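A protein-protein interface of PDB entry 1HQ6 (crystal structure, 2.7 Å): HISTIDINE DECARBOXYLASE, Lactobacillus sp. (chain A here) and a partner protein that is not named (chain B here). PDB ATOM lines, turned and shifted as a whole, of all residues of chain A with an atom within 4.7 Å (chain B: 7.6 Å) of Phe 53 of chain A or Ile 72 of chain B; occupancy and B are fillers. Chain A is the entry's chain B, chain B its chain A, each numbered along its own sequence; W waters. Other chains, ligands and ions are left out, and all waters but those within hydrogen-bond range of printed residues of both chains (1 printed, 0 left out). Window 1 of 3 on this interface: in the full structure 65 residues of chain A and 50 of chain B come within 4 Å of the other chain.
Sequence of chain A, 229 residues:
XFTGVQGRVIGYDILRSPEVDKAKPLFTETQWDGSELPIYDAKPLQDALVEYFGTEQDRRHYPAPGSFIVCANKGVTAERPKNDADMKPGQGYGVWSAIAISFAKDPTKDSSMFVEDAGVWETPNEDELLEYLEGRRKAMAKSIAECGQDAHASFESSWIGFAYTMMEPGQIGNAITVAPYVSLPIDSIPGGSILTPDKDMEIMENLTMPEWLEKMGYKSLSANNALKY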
ATOM      1  N   LEU A  49       6.277   4.170  -0.359  1.00  0.00           N
ATOM      2  CA  LEU A  49       5.151   4.642   0.433  1.00  0.00           C
ATOM      3  C   LEU A  49       4.917   6.126   0.239  1.00  0.00           C
ATOM      4  O   LEU A  49       3.774   6.580   0.146  1.00  0.00           O
ATOM      5  CB  LEU A  49       5.361   4.395   1.921  1.00  0.00           C
ATOM      6  CG  LEU A  49       4.201   4.768   2.842  1.00  0.00           C
ATOM      7  CD1 LEU A  49       2.969   3.977   2.452  1.00  0.00           C
ATOM      8  CD2 LEU A  49       4.546   4.447   4.283  1.00  0.00           C
ATOM      9  N   VAL A  50       5.997   6.886   0.139  1.00  0.00           N
ATOM     10  CA  VAL A  50       5.904   8.333  -0.014  1.00  0.00           C
ATOM     11  C   VAL A  50       5.218   8.635  -1.331  1.00  0.00           C
ATOM     12  O   VAL A  50       4.369   9.529  -1.401  1.00  0.00           O
ATOM     13  CB  VAL A  50       7.314   8.953   0.029  1.00  0.00           C
ATOM     14  CG1 VAL A  50       7.248  10.443  -0.205  1.00  0.00           C
ATOM     15  CG2 VAL A  50       7.924   8.726   1.403  1.00  0.00           C
ATOM     16  N   GLU A  51       5.583   7.860  -2.355  1.00  0.00           N
ATOM     17  CA  GLU A  51       4.929   7.946  -3.649  1.00  0.00           C
ATOM     18  C   GLU A  51       3.437   7.745  -3.555  1.00  0.00           C
ATOM     19  O   GLU A  51       2.684   8.588  -4.045  1.00  0.00           O
ATOM     20  CB  GLU A  51       5.448   6.903  -4.625  1.00  0.00           C
ATOM     21  CG  GLU A  51       6.864   7.123  -5.162  1.00  0.00           C
ATOM     22  CD  GLU A  51       7.061   8.341  -6.047  1.00  0.00           C
ATOM     23  OE1 GLU A  51       6.280   9.301  -6.006  1.00  0.00           O
ATOM     24  OE2 GLU A  51       8.038   8.316  -6.786  1.00  0.00           O
ATOM     25  N   TYR A  52       2.985   6.669  -2.910  1.00  0.00           N
ATOM     26  CA  TYR A  52       1.554   6.411  -2.820  1.00  0.00           C
ATOM     27  C   TYR A  52       0.785   7.386  -1.933  1.00  0.00           C
ATOM     28  O   TYR A  52      -0.285   7.844  -2.344  1.00  0.00           O
ATOM     29  CB  TYR A  52       1.315   5.009  -2.318  1.00  0.00           C
ATOM     30  CG  TYR A  52      -0.109   4.528  -2.508  1.00  0.00           C
ATOM     31  CD1 TYR A  52      -0.623   4.348  -3.791  1.00  0.00           C
ATOM     32  CD2 TYR A  52      -0.905   4.275  -1.399  1.00  0.00           C
ATOM     33  CE1 TYR A  52      -1.945   3.918  -3.962  1.00  0.00           C
ATOM     34  CE2 TYR A  52      -2.221   3.842  -1.562  1.00  0.00           C
ATOM     35  CZ  TYR A  52      -2.738   3.672  -2.840  1.00  0.00           C
ATOM     36  OH  TYR A  52      -4.060   3.307  -2.993  1.00  0.00           O
ATOM     37  N   PHE A  53       1.213   7.736  -0.724  1.00  0.00           N
ATOM     38  CA  PHE A  53       0.450   8.669   0.107  1.00  0.00           C
ATOM     39  C   PHE A  53       0.652  10.127  -0.269  1.00  0.00           C
ATOM     40  O   PHE A  53      -0.254  10.965  -0.153  1.00  0.00           O
ATOM     41  CB  PHE A  53       0.813   8.539   1.563  1.00  0.00           C
ATOM     42  CG  PHE A  53       0.360   7.284   2.267  1.00  0.00           C
ATOM     43  CD1 PHE A  53       0.691   7.137   3.608  1.00  0.00           C
ATOM     44  CD2 PHE A  53      -0.387   6.290   1.634  1.00  0.00           C
ATOM     45  CE1 PHE A  53       0.288   6.010   4.314  1.00  0.00           C
ATOM     46  CE2 PHE A  53      -0.791   5.166   2.340  1.00  0.00           C
ATOM     47  CZ  PHE A  53      -0.454   5.026   3.679  1.00  0.00           C
ATOM     48  N   GLY A  54       1.850  10.441  -0.771  1.00  0.00           N
ATOM     49  CA  GLY A  54       2.210  11.798  -1.130  1.00  0.00           C
ATOM     50  C   GLY A  54       2.727  12.498   0.113  1.00  0.00           C
ATOM     51  O   GLY A  54       2.912  11.902   1.188  1.00  0.00           O
ATOM     52  N   THR A  55       2.952  13.796  -0.044  1.00  0.00           N
ATOM     53  CA  THR A  55       3.509  14.592   1.022  1.00  0.00           C
ATOM     54  C   THR A  55       2.531  15.667   1.438  1.00  0.00           C
ATOM     55  O   THR A  55       1.676  16.080   0.664  1.00  0.00           O
ATOM     56  CB  THR A  55       4.828  15.206   0.541  1.00  0.00           C
ATOM     57  OG1 THR A  55       4.583  15.992  -0.623  1.00  0.00           O
ATOM     58  CG2 THR A  55       5.840  14.120   0.225  1.00  0.00           C
ATOM     59  N   ARG A  59      -0.411  16.141  -1.531  1.00  0.00           N
ATOM     60  CA  ARG A  59      -1.107  15.019  -0.940  1.00  0.00           C
ATOM     61  C   ARG A  59      -1.727  14.100  -2.000  1.00  0.00           C
ATOM     62  O   ARG A  59      -2.445  14.595  -2.874  1.00  0.00           O
ATOM     63  CB  ARG A  59      -2.208  15.545   0.001  1.00  0.00           C
ATOM     64  CG  ARG A  59      -1.750  16.383   1.181  1.00  0.00           C
ATOM     65  CD  ARG A  59      -2.904  16.740   2.103  1.00  0.00           C
ATOM     66  NE  ARG A  59      -2.505  17.753   3.068  1.00  0.00           N
ATOM     67  CZ  ARG A  59      -3.280  18.126   4.095  1.00  0.00           C
ATOM     68  NH1 ARG A  59      -2.862  19.069   4.944  1.00  0.00           N
ATOM     69  NH2 ARG A  59      -4.468  17.555   4.328  1.00  0.00           N
ATOM     70  N   ARG A  60      -1.468  12.789  -1.961  1.00  0.00           N
ATOM     71  CA  ARG A  60      -2.061  11.821  -2.868  1.00  0.00           C
ATOM     72  C   ARG A  60      -3.022  10.854  -2.152  1.00  0.00           C
ATOM     73  O   ARG A  60      -4.076  11.305  -1.678  1.00  0.00           O
ATOM     74  CB  ARG A  60      -0.951  11.050  -3.554  1.00  0.00           C
ATOM     75  CG  ARG A  60      -0.188  11.941  -4.510  1.00  0.00           C
ATOM     76  CD  ARG A  60       1.029  11.212  -5.056  1.00  0.00           C
ATOM     77  NE  ARG A  60       1.778  12.112  -5.900  1.00  0.00           N
ATOM     78  CZ  ARG A  60       2.879  11.747  -6.535  1.00  0.00           C
ATOM     79  NH1 ARG A  60       3.496  12.656  -7.286  1.00  0.00           N
ATOM     80  NH2 ARG A  60       3.370  10.511  -6.464  1.00  0.00           N
ATOM     81  N   HIS A  61      -2.792   9.536  -2.004  1.00  0.00           N
ATOM     82  CA  HIS A  61      -3.778   8.645  -1.394  1.00  0.00           C
ATOM     83  C   HIS A  61      -3.581   8.449   0.086  1.00  0.00           C
ATOM     84  O   HIS A  61      -3.428   7.343   0.616  1.00  0.00           O
ATOM     85  CB  HIS A  61      -3.739   7.309  -2.095  1.00  0.00           C
ATOM     86  CG  HIS A  61      -3.991   7.581  -3.555  1.00  0.00           C
ATOM     87  ND1 HIS A  61      -5.040   8.214  -4.063  1.00  0.00           N
ATOM     88  CD2 HIS A  61      -3.115   7.306  -4.572  1.00  0.00           C
ATOM     89  CE1 HIS A  61      -4.825   8.351  -5.344  1.00  0.00           C
ATOM     90  NE2 HIS A  61      -3.674   7.801  -5.637  1.00  0.00           N
ATOM     91  N   TYR A  62      -3.600   9.580   0.772  1.00  0.00           N
ATOM     92  CA  TYR A  62      -3.346   9.575   2.199  1.00  0.00           C
ATOM     93  C   TYR A  62      -4.562   9.045   2.893  1.00  0.00           C
ATOM     94  O   TYR A  62      -5.668   9.162   2.373  1.00  0.00           O
ATOM     95  CB  TYR A  62      -3.030  10.987   2.723  1.00  0.00           C
ATOM     96  CG  TYR A  62      -4.088  12.058   2.548  1.00  0.00           C
ATOM     97  CD1 TYR A  62      -4.353  12.587   1.295  1.00  0.00           C
ATOM     98  CD2 TYR A  62      -4.771  12.533   3.660  1.00  0.00           C
ATOM     99  CE1 TYR A  62      -5.294  13.607   1.148  1.00  0.00           C
ATOM    100  CE2 TYR A  62      -5.713  13.550   3.524  1.00  0.00           C
ATOM    101  CZ  TYR A  62      -5.967  14.089   2.261  1.00  0.00           C
ATOM    102  OH  TYR A  62      -6.872  15.129   2.104  1.00  0.00           O
ATOM    103  N   PRO A  63      -4.449   8.434   4.047  1.00  0.00           N
ATOM    104  CA  PRO A  63      -5.589   7.985   4.814  1.00  0.00           C
ATOM    105  C   PRO A  63      -6.550   9.098   5.195  1.00  0.00           C
ATOM    106  O   PRO A  63      -6.209  10.201   5.619  1.00  0.00           O
ATOM    107  CB  PRO A  63      -4.946   7.270   5.980  1.00  0.00           C
ATOM    108  CG  PRO A  63      -3.553   7.817   6.049  1.00  0.00           C
ATOM    109  CD  PRO A  63      -3.215   7.901   4.582  1.00  0.00           C
ATOM    110  N   ILE A 176       9.731   8.487  14.467  1.00  0.00           N
ATOM    111  CA  ILE A 176       8.667   7.484  14.531  1.00  0.00           C
ATOM    112  C   ILE A 176       8.927   6.347  13.568  1.00  0.00           C
ATOM    113  O   ILE A 176       9.557   6.553  12.527  1.00  0.00           O
ATOM    114  CB  ILE A 176       7.309   8.081  14.174  1.00  0.00           C
ATOM    115  CG1 ILE A 176       7.349   8.668  12.766  1.00  0.00           C
ATOM    116  CG2 ILE A 176       6.942   9.160  15.161  1.00  0.00           C
ATOM    117  CD1 ILE A 176       5.936   8.892  12.195  1.00  0.00           C
ATOM    118  N   VAL A 178       6.573   3.429  11.740  1.00  0.00           N
ATOM    119  CA  VAL A 178       5.183   3.025  11.562  1.00  0.00           C
ATOM    120  C   VAL A 178       4.958   2.250  10.277  1.00  0.00           C
ATOM    121  O   VAL A 178       5.500   2.593   9.223  1.00  0.00           O
ATOM    122  CB  VAL A 178       4.304   4.298  11.611  1.00  0.00           C
ATOM    123  CG1 VAL A 178       4.814   5.292  10.617  1.00  0.00           C
ATOM    124  CG2 VAL A 178       2.878   4.012  11.219  1.00  0.00           C
ATOM    125  N   PRO A 180       1.495   0.940   8.385  1.00  0.00           N
ATOM    126  CA  PRO A 180       0.048   1.044   8.460  1.00  0.00           C
ATOM    127  C   PRO A 180      -0.639  -0.105   7.754  1.00  0.00           C
ATOM    128  O   PRO A 180      -0.054  -0.706   6.852  1.00  0.00           O
ATOM    129  CB  PRO A 180      -0.213   2.368   7.851  1.00  0.00           C
ATOM    130  CG  PRO A 180       0.738   2.375   6.704  1.00  0.00           C
ATOM    131  CD  PRO A 180       1.991   1.805   7.325  1.00  0.00           C
ATOM    132  N   VAL A 182      -3.746  -0.702   5.532  1.00  0.00           N
ATOM    133  CA  VAL A 182      -4.790   0.041   4.845  1.00  0.00           C
ATOM    134  C   VAL A 182      -5.481  -0.708   3.718  1.00  0.00           C
ATOM    135  O   VAL A 182      -5.077  -1.816   3.354  1.00  0.00           O
ATOM    136  CB  VAL A 182      -4.171   1.333   4.296  1.00  0.00           C
ATOM    137  CG1 VAL A 182      -3.659   2.206   5.423  1.00  0.00           C
ATOM    138  CG2 VAL A 182      -3.028   0.985   3.363  1.00  0.00           C
ATOM    139  N   GLN B  22     -10.149   9.251  -3.467  1.00  0.00           N
ATOM    140  CA  GLN B  22      -8.773   9.617  -3.131  1.00  0.00           C
ATOM    141  C   GLN B  22      -8.152   8.903  -1.947  1.00  0.00           C
ATOM    142  O   GLN B  22      -7.062   8.364  -2.100  1.00  0.00           O
ATOM    143  CB  GLN B  22      -8.640  11.125  -2.881  1.00  0.00           C
ATOM    144  CG  GLN B  22      -7.193  11.631  -2.817  1.00  0.00           C
ATOM    145  CD  GLN B  22      -7.029  13.138  -2.598  1.00  0.00           C
ATOM    146  OE1 GLN B  22      -7.997  13.910  -2.572  1.00  0.00           O
ATOM    147  NE2 GLN B  22      -5.814  13.661  -2.419  1.00  0.00           N
ATOM    148  N   THR B  24      -7.234   6.448   1.373  1.00  0.00           N
ATOM    149  CA  THR B  24      -7.120   5.064   1.814  1.00  0.00           C
ATOM    150  C   THR B  24      -7.853   5.044   3.133  1.00  0.00           C
ATOM    151  O   THR B  24      -8.057   6.079   3.791  1.00  0.00           O
ATOM    152  CB  THR B  24      -5.685   4.643   2.097  1.00  0.00           C
ATOM    153  OG1 THR B  24      -5.035   5.801   2.622  1.00  0.00           O
ATOM    154  CG2 THR B  24      -4.945   4.169   0.892  1.00  0.00           C
ATOM    155  N   ARG B  25      -8.241   3.857   3.544  1.00  0.00           N
ATOM    156  CA  ARG B  25      -8.850   3.634   4.840  1.00  0.00           C
ATOM    157  C   ARG B  25      -8.036   2.550   5.517  1.00  0.00           C
ATOM    158  O   ARG B  25      -7.100   2.005   4.926  1.00  0.00           O
ATOM    159  CB  ARG B  25     -10.276   3.170   4.683  1.00  0.00           C
ATOM    160  CG  ARG B  25     -11.172   4.247   4.146  1.00  0.00           C
ATOM    161  CD  ARG B  25     -12.513   3.604   3.948  1.00  0.00           C
ATOM    162  NE  ARG B  25     -13.414   3.824   5.052  1.00  0.00           N
ATOM    163  CZ  ARG B  25     -14.311   2.902   5.398  1.00  0.00           C
ATOM    164  NH1 ARG B  25     -15.120   3.163   6.409  1.00  0.00           N
ATOM    165  NH2 ARG B  25     -14.400   1.718   4.786  1.00  0.00           N
ATOM    166  N   VAL B  38      -3.084  -3.915   3.088  1.00  0.00           N
ATOM    167  CA  VAL B  38      -1.885  -3.567   2.376  1.00  0.00           C
ATOM    168  C   VAL B  38      -1.073  -2.732   3.354  1.00  0.00           C
ATOM    169  O   VAL B  38      -1.626  -1.902   4.076  1.00  0.00           O
ATOM    170  CB  VAL B  38      -2.314  -2.818   1.138  1.00  0.00           C
ATOM    171  CG1 VAL B  38      -1.140  -2.233   0.397  1.00  0.00           C
ATOM    172  CG2 VAL B  38      -2.937  -3.799   0.208  1.00  0.00           C
ATOM    173  N   THR B  39       0.222  -2.965   3.442  1.00  0.00           N
ATOM    174  CA  THR B  39       1.036  -2.261   4.396  1.00  0.00           C
ATOM    175  C   THR B  39       2.231  -1.637   3.690  1.00  0.00           C
ATOM    176  O   THR B  39       2.566  -1.961   2.544  1.00  0.00           O
ATOM    177  CB  THR B  39       1.409  -3.282   5.474  1.00  0.00           C
ATOM    178  OG1 THR B  39       2.091  -2.559   6.470  1.00  0.00           O
ATOM    179  CG2 THR B  39       2.245  -4.423   4.977  1.00  0.00           C
ATOM    180  N   GLY B  40       2.892  -0.730   4.396  1.00  0.00           N
ATOM    181  CA  GLY B  40       4.065  -0.012   3.911  1.00  0.00           C
ATOM    182  C   GLY B  40       4.998   0.365   5.052  1.00  0.00           C
ATOM    183  O   GLY B  40       4.699   0.111   6.215  1.00  0.00           O
ATOM    184  N   LYS B  42       7.210   3.357   7.063  1.00  0.00           N
ATOM    185  CA  LYS B  42       7.536   4.750   7.261  1.00  0.00           C
ATOM    186  C   LYS B  42       8.384   4.921   8.509  1.00  0.00           C
ATOM    187  O   LYS B  42       7.985   4.565   9.612  1.00  0.00           O
ATOM    188  CB  LYS B  42       6.270   5.578   7.410  1.00  0.00           C
ATOM    189  CG  LYS B  42       6.518   7.057   7.726  1.00  0.00           C
ATOM    190  CD  LYS B  42       5.230   7.843   7.860  1.00  0.00           C
ATOM    191  CE  LYS B  42       5.498   9.224   8.440  1.00  0.00           C
ATOM    192  NZ  LYS B  42       6.319  10.043   7.576  1.00  0.00           N
ATOM    193  N   ALA B  65       7.044  14.811  12.935  1.00  0.00           N
ATOM    194  CA  ALA B  65       7.579  13.647  12.219  1.00  0.00           C
ATOM    195  C   ALA B  65       6.511  13.064  11.282  1.00  0.00           C
ATOM    196  O   ALA B  65       6.728  13.020  10.079  1.00  0.00           O
ATOM    197  CB  ALA B  65       8.003  12.568  13.199  1.00  0.00           C
ATOM    198  N   GLU B  66       5.285  12.778  11.768  1.00  0.00           N
ATOM    199  CA  GLU B  66       4.174  12.240  10.958  1.00  0.00           C
ATOM    200  C   GLU B  66       3.819  13.016   9.695  1.00  0.00           C
ATOM    201  O   GLU B  66       3.198  12.504   8.757  1.00  0.00           O
ATOM    202  CB  GLU B  66       2.809  12.160  11.674  1.00  0.00           C
ATOM    203  CG  GLU B  66       2.601  12.506  13.137  1.00  0.00           C
ATOM    204  CD  GLU B  66       3.412  11.630  14.083  1.00  0.00           C
ATOM    205  OE1 GLU B  66       4.268  12.154  14.807  1.00  0.00           O
ATOM    206  OE2 GLU B  66       3.185  10.422  14.092  1.00  0.00           O
ATOM    207  N   THR B  67       4.134  14.299   9.662  1.00  0.00           N
ATOM    208  CA  THR B  67       3.761  15.072   8.501  1.00  0.00           C
ATOM    209  C   THR B  67       4.912  15.195   7.504  1.00  0.00           C
ATOM    210  O   THR B  67       4.744  15.772   6.417  1.00  0.00           O
ATOM    211  CB  THR B  67       3.214  16.402   9.100  1.00  0.00           C
ATOM    212  OG1 THR B  67       3.972  16.796  10.260  1.00  0.00           O
ATOM    213  CG2 THR B  67       1.767  16.194   9.536  1.00  0.00           C
ATOM    214  N   LYS B  68       6.087  14.661   7.858  1.00  0.00           N
ATOM    215  CA  LYS B  68       7.246  14.733   6.985  1.00  0.00           C
ATOM    216  C   LYS B  68       7.121  13.597   5.993  1.00  0.00           C
ATOM    217  O   LYS B  68       6.769  12.475   6.358  1.00  0.00           O
ATOM    218  CB  LYS B  68       8.621  14.467   7.629  1.00  0.00           C
ATOM    219  CG  LYS B  68       9.222  15.454   8.630  1.00  0.00           C
ATOM    220  CD  LYS B  68      10.623  15.019   9.112  1.00  0.00           C
ATOM    221  CE  LYS B  68      11.811  15.373   8.187  1.00  0.00           C
ATOM    222  NZ  LYS B  68      11.933  14.515   7.010  1.00  0.00           N
ATOM    223  N   ASN B  69       7.528  13.835   4.749  1.00  0.00           N
ATOM    224  CA  ASN B  69       7.524  12.805   3.741  1.00  0.00           C
ATOM    225  C   ASN B  69       6.158  12.142   3.641  1.00  0.00           C
ATOM    226  O   ASN B  69       5.211  12.886   3.368  1.00  0.00           O
ATOM    227  CB  ASN B  69       8.619  11.785   4.061  1.00  0.00           C
ATOM    228  CG  ASN B  69      10.015  12.312   3.743  1.00  0.00           C
ATOM    229  OD1 ASN B  69      10.192  13.042   2.762  1.00  0.00           O
ATOM    230  ND2 ASN B  69      11.061  11.982   4.505  1.00  0.00           N
ATOM    231  N   ALA B  70       5.953  10.843   3.901  1.00  0.00           N
ATOM    232  CA  ALA B  70       4.680  10.184   3.624  1.00  0.00           C
ATOM    233  C   ALA B  70       3.632  10.717   4.552  1.00  0.00           C
ATOM    234  O   ALA B  70       3.680  10.476   5.759  1.00  0.00           O
ATOM    235  CB  ALA B  70       4.780   8.692   3.851  1.00  0.00           C
ATOM    236  N   TYR B  71       2.663  11.405   4.002  1.00  0.00           N
ATOM    237  CA  TYR B  71       1.695  12.030   4.859  1.00  0.00           C
ATOM    238  C   TYR B  71       0.714  11.064   5.507  1.00  0.00           C
ATOM    239  O   TYR B  71      -0.222  10.583   4.871  1.00  0.00           O
ATOM    240  CB  TYR B  71       0.973  13.086   4.030  1.00  0.00           C
ATOM    241  CG  TYR B  71       0.007  13.964   4.804  1.00  0.00           C
ATOM    242  CD1 TYR B  71       0.448  14.743   5.879  1.00  0.00           C
ATOM    243  CD2 TYR B  71      -1.336  13.979   4.440  1.00  0.00           C
ATOM    244  CE1 TYR B  71      -0.460  15.530   6.594  1.00  0.00           C
ATOM    245  CE2 TYR B  71      -2.246  14.767   5.148  1.00  0.00           C
ATOM    246  CZ  TYR B  71      -1.803  15.534   6.224  1.00  0.00           C
ATOM    247  OH  TYR B  71      -2.693  16.283   6.959  1.00  0.00           O
ATOM    248  N   ILE B  72       0.890  10.681   6.760  1.00  0.00           N
ATOM    249  CA  ILE B  72      -0.149   9.909   7.422  1.00  0.00           C
ATOM    250  C   ILE B  72      -0.867  11.015   8.165  1.00  0.00           C
ATOM    251  O   ILE B  72      -0.469  11.483   9.222  1.00  0.00           O
ATOM    252  CB  ILE B  72       0.413   8.823   8.396  1.00  0.00           C
ATOM    253  CG1 ILE B  72       1.472   9.285   9.389  1.00  0.00           C
ATOM    254  CG2 ILE B  72       1.020   7.773   7.477  1.00  0.00           C
ATOM    255  CD1 ILE B  72       1.772   8.143  10.385  1.00  0.00           C
ATOM    256  N   GLY B  73      -1.901  11.479   7.487  1.00  0.00           N
ATOM    257  CA  GLY B  73      -2.687  12.630   7.872  1.00  0.00           C
ATOM    258  C   GLY B  73      -3.190  12.775   9.280  1.00  0.00           C
ATOM    259  O   GLY B  73      -2.525  12.547  10.271  1.00  0.00           O
ATOM    260  N   GLN B  74      -4.422  13.208   9.382  1.00  0.00           N
ATOM    261  CA  GLN B  74      -5.045  13.413  10.667  1.00  0.00           C
ATOM    262  C   GLN B  74      -5.774  12.086  10.858  1.00  0.00           C
ATOM    263  O   GLN B  74      -6.942  11.894  10.527  1.00  0.00           O
ATOM    264  CB  GLN B  74      -5.975  14.580  10.547  1.00  0.00           C
ATOM    265  CG  GLN B  74      -5.343  15.834   9.940  1.00  0.00           C
ATOM    266  CD  GLN B  74      -6.362  16.940   9.692  1.00  0.00           C
ATOM    267  OE1 GLN B  74      -6.830  17.154   8.586  1.00  0.00           O
ATOM    268  NE2 GLN B  74      -6.870  17.676  10.667  1.00  0.00           N
ATOM    269  N   ILE B  75      -5.025  11.140  11.385  1.00  0.00           N
ATOM    270  CA  ILE B  75      -5.396   9.753  11.529  1.00  0.00           C
ATOM    271  C   ILE B  75      -5.464   9.313  12.977  1.00  0.00           C
ATOM    272  O   ILE B  75      -4.803   9.887  13.831  1.00  0.00           O
ATOM    273  CB  ILE B  75      -4.343   9.021  10.663  1.00  0.00           C
ATOM    274  CG1 ILE B  75      -5.182   8.340   9.633  1.00  0.00           C
ATOM    275  CG2 ILE B  75      -3.405   8.058  11.377  1.00  0.00           C
ATOM    276  CD1 ILE B  75      -5.923   9.316   8.709  1.00  0.00           C
ATOM    277  N   MET B  77      -4.545   6.254  15.198  1.00  0.00           N
ATOM    278  CA  MET B  77      -3.900   4.976  15.026  1.00  0.00           C
ATOM    279  C   MET B  77      -4.123   4.137  16.250  1.00  0.00           C
ATOM    280  O   MET B  77      -4.460   4.681  17.301  1.00  0.00           O
ATOM    281  CB  MET B  77      -2.421   5.147  14.753  1.00  0.00           C
ATOM    282  CG  MET B  77      -1.507   5.892  15.684  1.00  0.00           C
ATOM    283  SD  MET B  77       0.046   5.929  14.767  1.00  0.00           S
ATOM    284  CE  MET B  77       0.086   7.656  14.368  1.00  0.00           C
HETATM  285  O   HOH W   1      -5.928  12.455   6.881  1.00  0.00           O
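Among the printed residues, merely in contact across the chains: Leu 49 of chain A with Lys 42 of chain B (3.7 Å), Val 50 of chain A with Ala 70 of chain B (3.8 Å), Tyr 52 of chain A with Thr 24 of chain B (3.7 Å), Phe 53 of chain A with Tyr 71 of chain B (3.8 Å), Phe 53 of chain A with Ile 72 of chain B (3.7 Å), Gly 54 of chain A with Ala 70 of chain B (3.5 Å), Thr 55 of chain A with Asn 69 of chain B (3.4 Å), Thr 55 of chain A with Tyr 71 of chain B (3.98 Å), Arg 59 of chain A with Gln 22 of chain B (3.5 Å), Tyr 62 of chain A with Gln 22 of chain B (3.6 Å), Tyr 62 of chain A with Tyr 71 of chain B (3.6 Å), Pro 63 of chain A with Ile 75 of chain B (3.2 Å), Ile 176 of chain A with Lys 42 of chain B (3.8 Å), Ile 176 of chain A with Ala 65 of chain B (3.98 Å), Ile 176 of chain A with Glu 66 of chain B (3.7 Å), Val 178 of chain A with Gly 40 of chain B (3.98 Å), Pro 180 of chain A with Gly 40 of chain B (3.4 Å) and Val 182 of chain A with Arg 25 of chain B (3.0 Å).
N of Val 182 of chain A sits at hydrogen-bond distance from O of Val 38 of chain B, at 2.8 Å. The side-chain hydroxyl of Thr 24 of chain B sits at hydrogen-bond distance from the backbone carbonyl oxygen of His 61 of chain A. O of Asn 69 of chain B lies close to O of Gly 54 of chain A (3.3 Å). O of Gly 54 of chain A is in hydrogen-bond range of N of Tyr 71 of chain B. N of Thr 24 of chain B lies within hydrogen-bond range of O of Tyr 62 of chain A, at 3.3 Å. O of Pro 180 of chain A sits at hydrogen-bond distance from OG1 of Thr 39 of chain B (2.9 Å). The backbone carbonyl oxygen (O) of Pro 180 of chain A sits close to the backbone carbonyl oxygen (O) of Val 38 of chain B (3.4 Å). O of Gln 22 of chain B is in hydrogen-bond range of ND1 of His 61 of chain A (2.8 Å). NE2 of Gln 22 of chain B lies within hydrogen-bond range of O of Arg 60 of chain A, 3.0 Å away. N of Pro 63 of chain A sits close to OG1 of Thr 24 of chain B (3.1 Å). OH of Tyr 71 of chain B is in hydrogen-bond range of NH2 of Arg 59 of chain A (3.4 Å). The backbone carbonyl oxygen of Lys 42 of chain B sits at hydrogen-bond distance from the backbone NH of Val 178 of chain A (2.8 Å).
O of Ala 70 of chain B is in hydrogen-bond range of NZ of Lys 42 of chain B (3.2 Å). The backbone carbonyl oxygen of Phe 53 of chain A sits at hydrogen-bond distance from the backbone NH of His 61 of chain A (3.5 Å). NZ of Lys 42 of chain B lies within hydrogen-bond range of O of Lys 68 of chain B (2.8 Å). NH2 of Arg 60 of chain A is in salt-bridge range of OE1 of Glu 51 of chain A. N of His 61 of chain A is in hydrogen-bond range of O of Tyr 52 of chain A (3.0 Å). The backbone carbonyl oxygen of Phe 53 of chain A sits at hydrogen-bond distance from the backbone NH of Arg 60 of chain A, 2.8 Å away.
Of the 16 printed residues of chain A, 15 touch a printed residue of chain B. Hydrophobic or aromatic side chains of chain A within 4 Å of the printed part of chain B: Leu 49, Val 50, Tyr 52, Phe 53, His 61, Tyr 62, Pro 63, Ile 176, Val 178, Pro 180 and Val 182. Printed residues of chain B that touch a printed residue of chain A: Gln 22, Thr 24, Arg 25, Val 38, Thr 39, Gly 40, Lys 42, Ala 65, Glu 66, Asn 69, Ala 70, Tyr 71, Ile 72 and Ile 75. Hydrophobic or aromatic side chains of chain B that line the printed part of chain A: Val 38, Ala 65, Ala 70, Tyr 71, Ile 72 and Ile 75. Among the printed residues, 30 pairs touch across the chains.
Water W1 lies within hydrogen-bond range of O of Pro 63 of chain A and N of Gln 74 of chain B.
Phe 53 of chain A touches just these residues of chain B: Tyr 71 (3.8 Å) and Ile 72 (3.7 Å). Of chain A, only Phe 53 (3.7 Å) comes within 4 Å of Ile 72 of chain B. Of the printed residues of chain B, Gly 54 of chain A touches Asn 69 (3.3 Å), Ala 70 (3.5 Å) and Tyr 71 (2.9 Å). Printed residues of chain B within 4 Å of Arg 60 of chain A: Gln 22. Of the printed residues of chain B, Thr 55 of chain A touches Asn 69 and Tyr 71. Thr 67 of chain B touches none of the printed residues of chain A. The nearest residue of chain A that does not touch Ile 72 of chain B is Val 178 of chain A (4.2 Å). The nearest printed residue of chain B that does not touch Tyr 52 of chain A is Gln 22 of chain B (5.9 Å).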
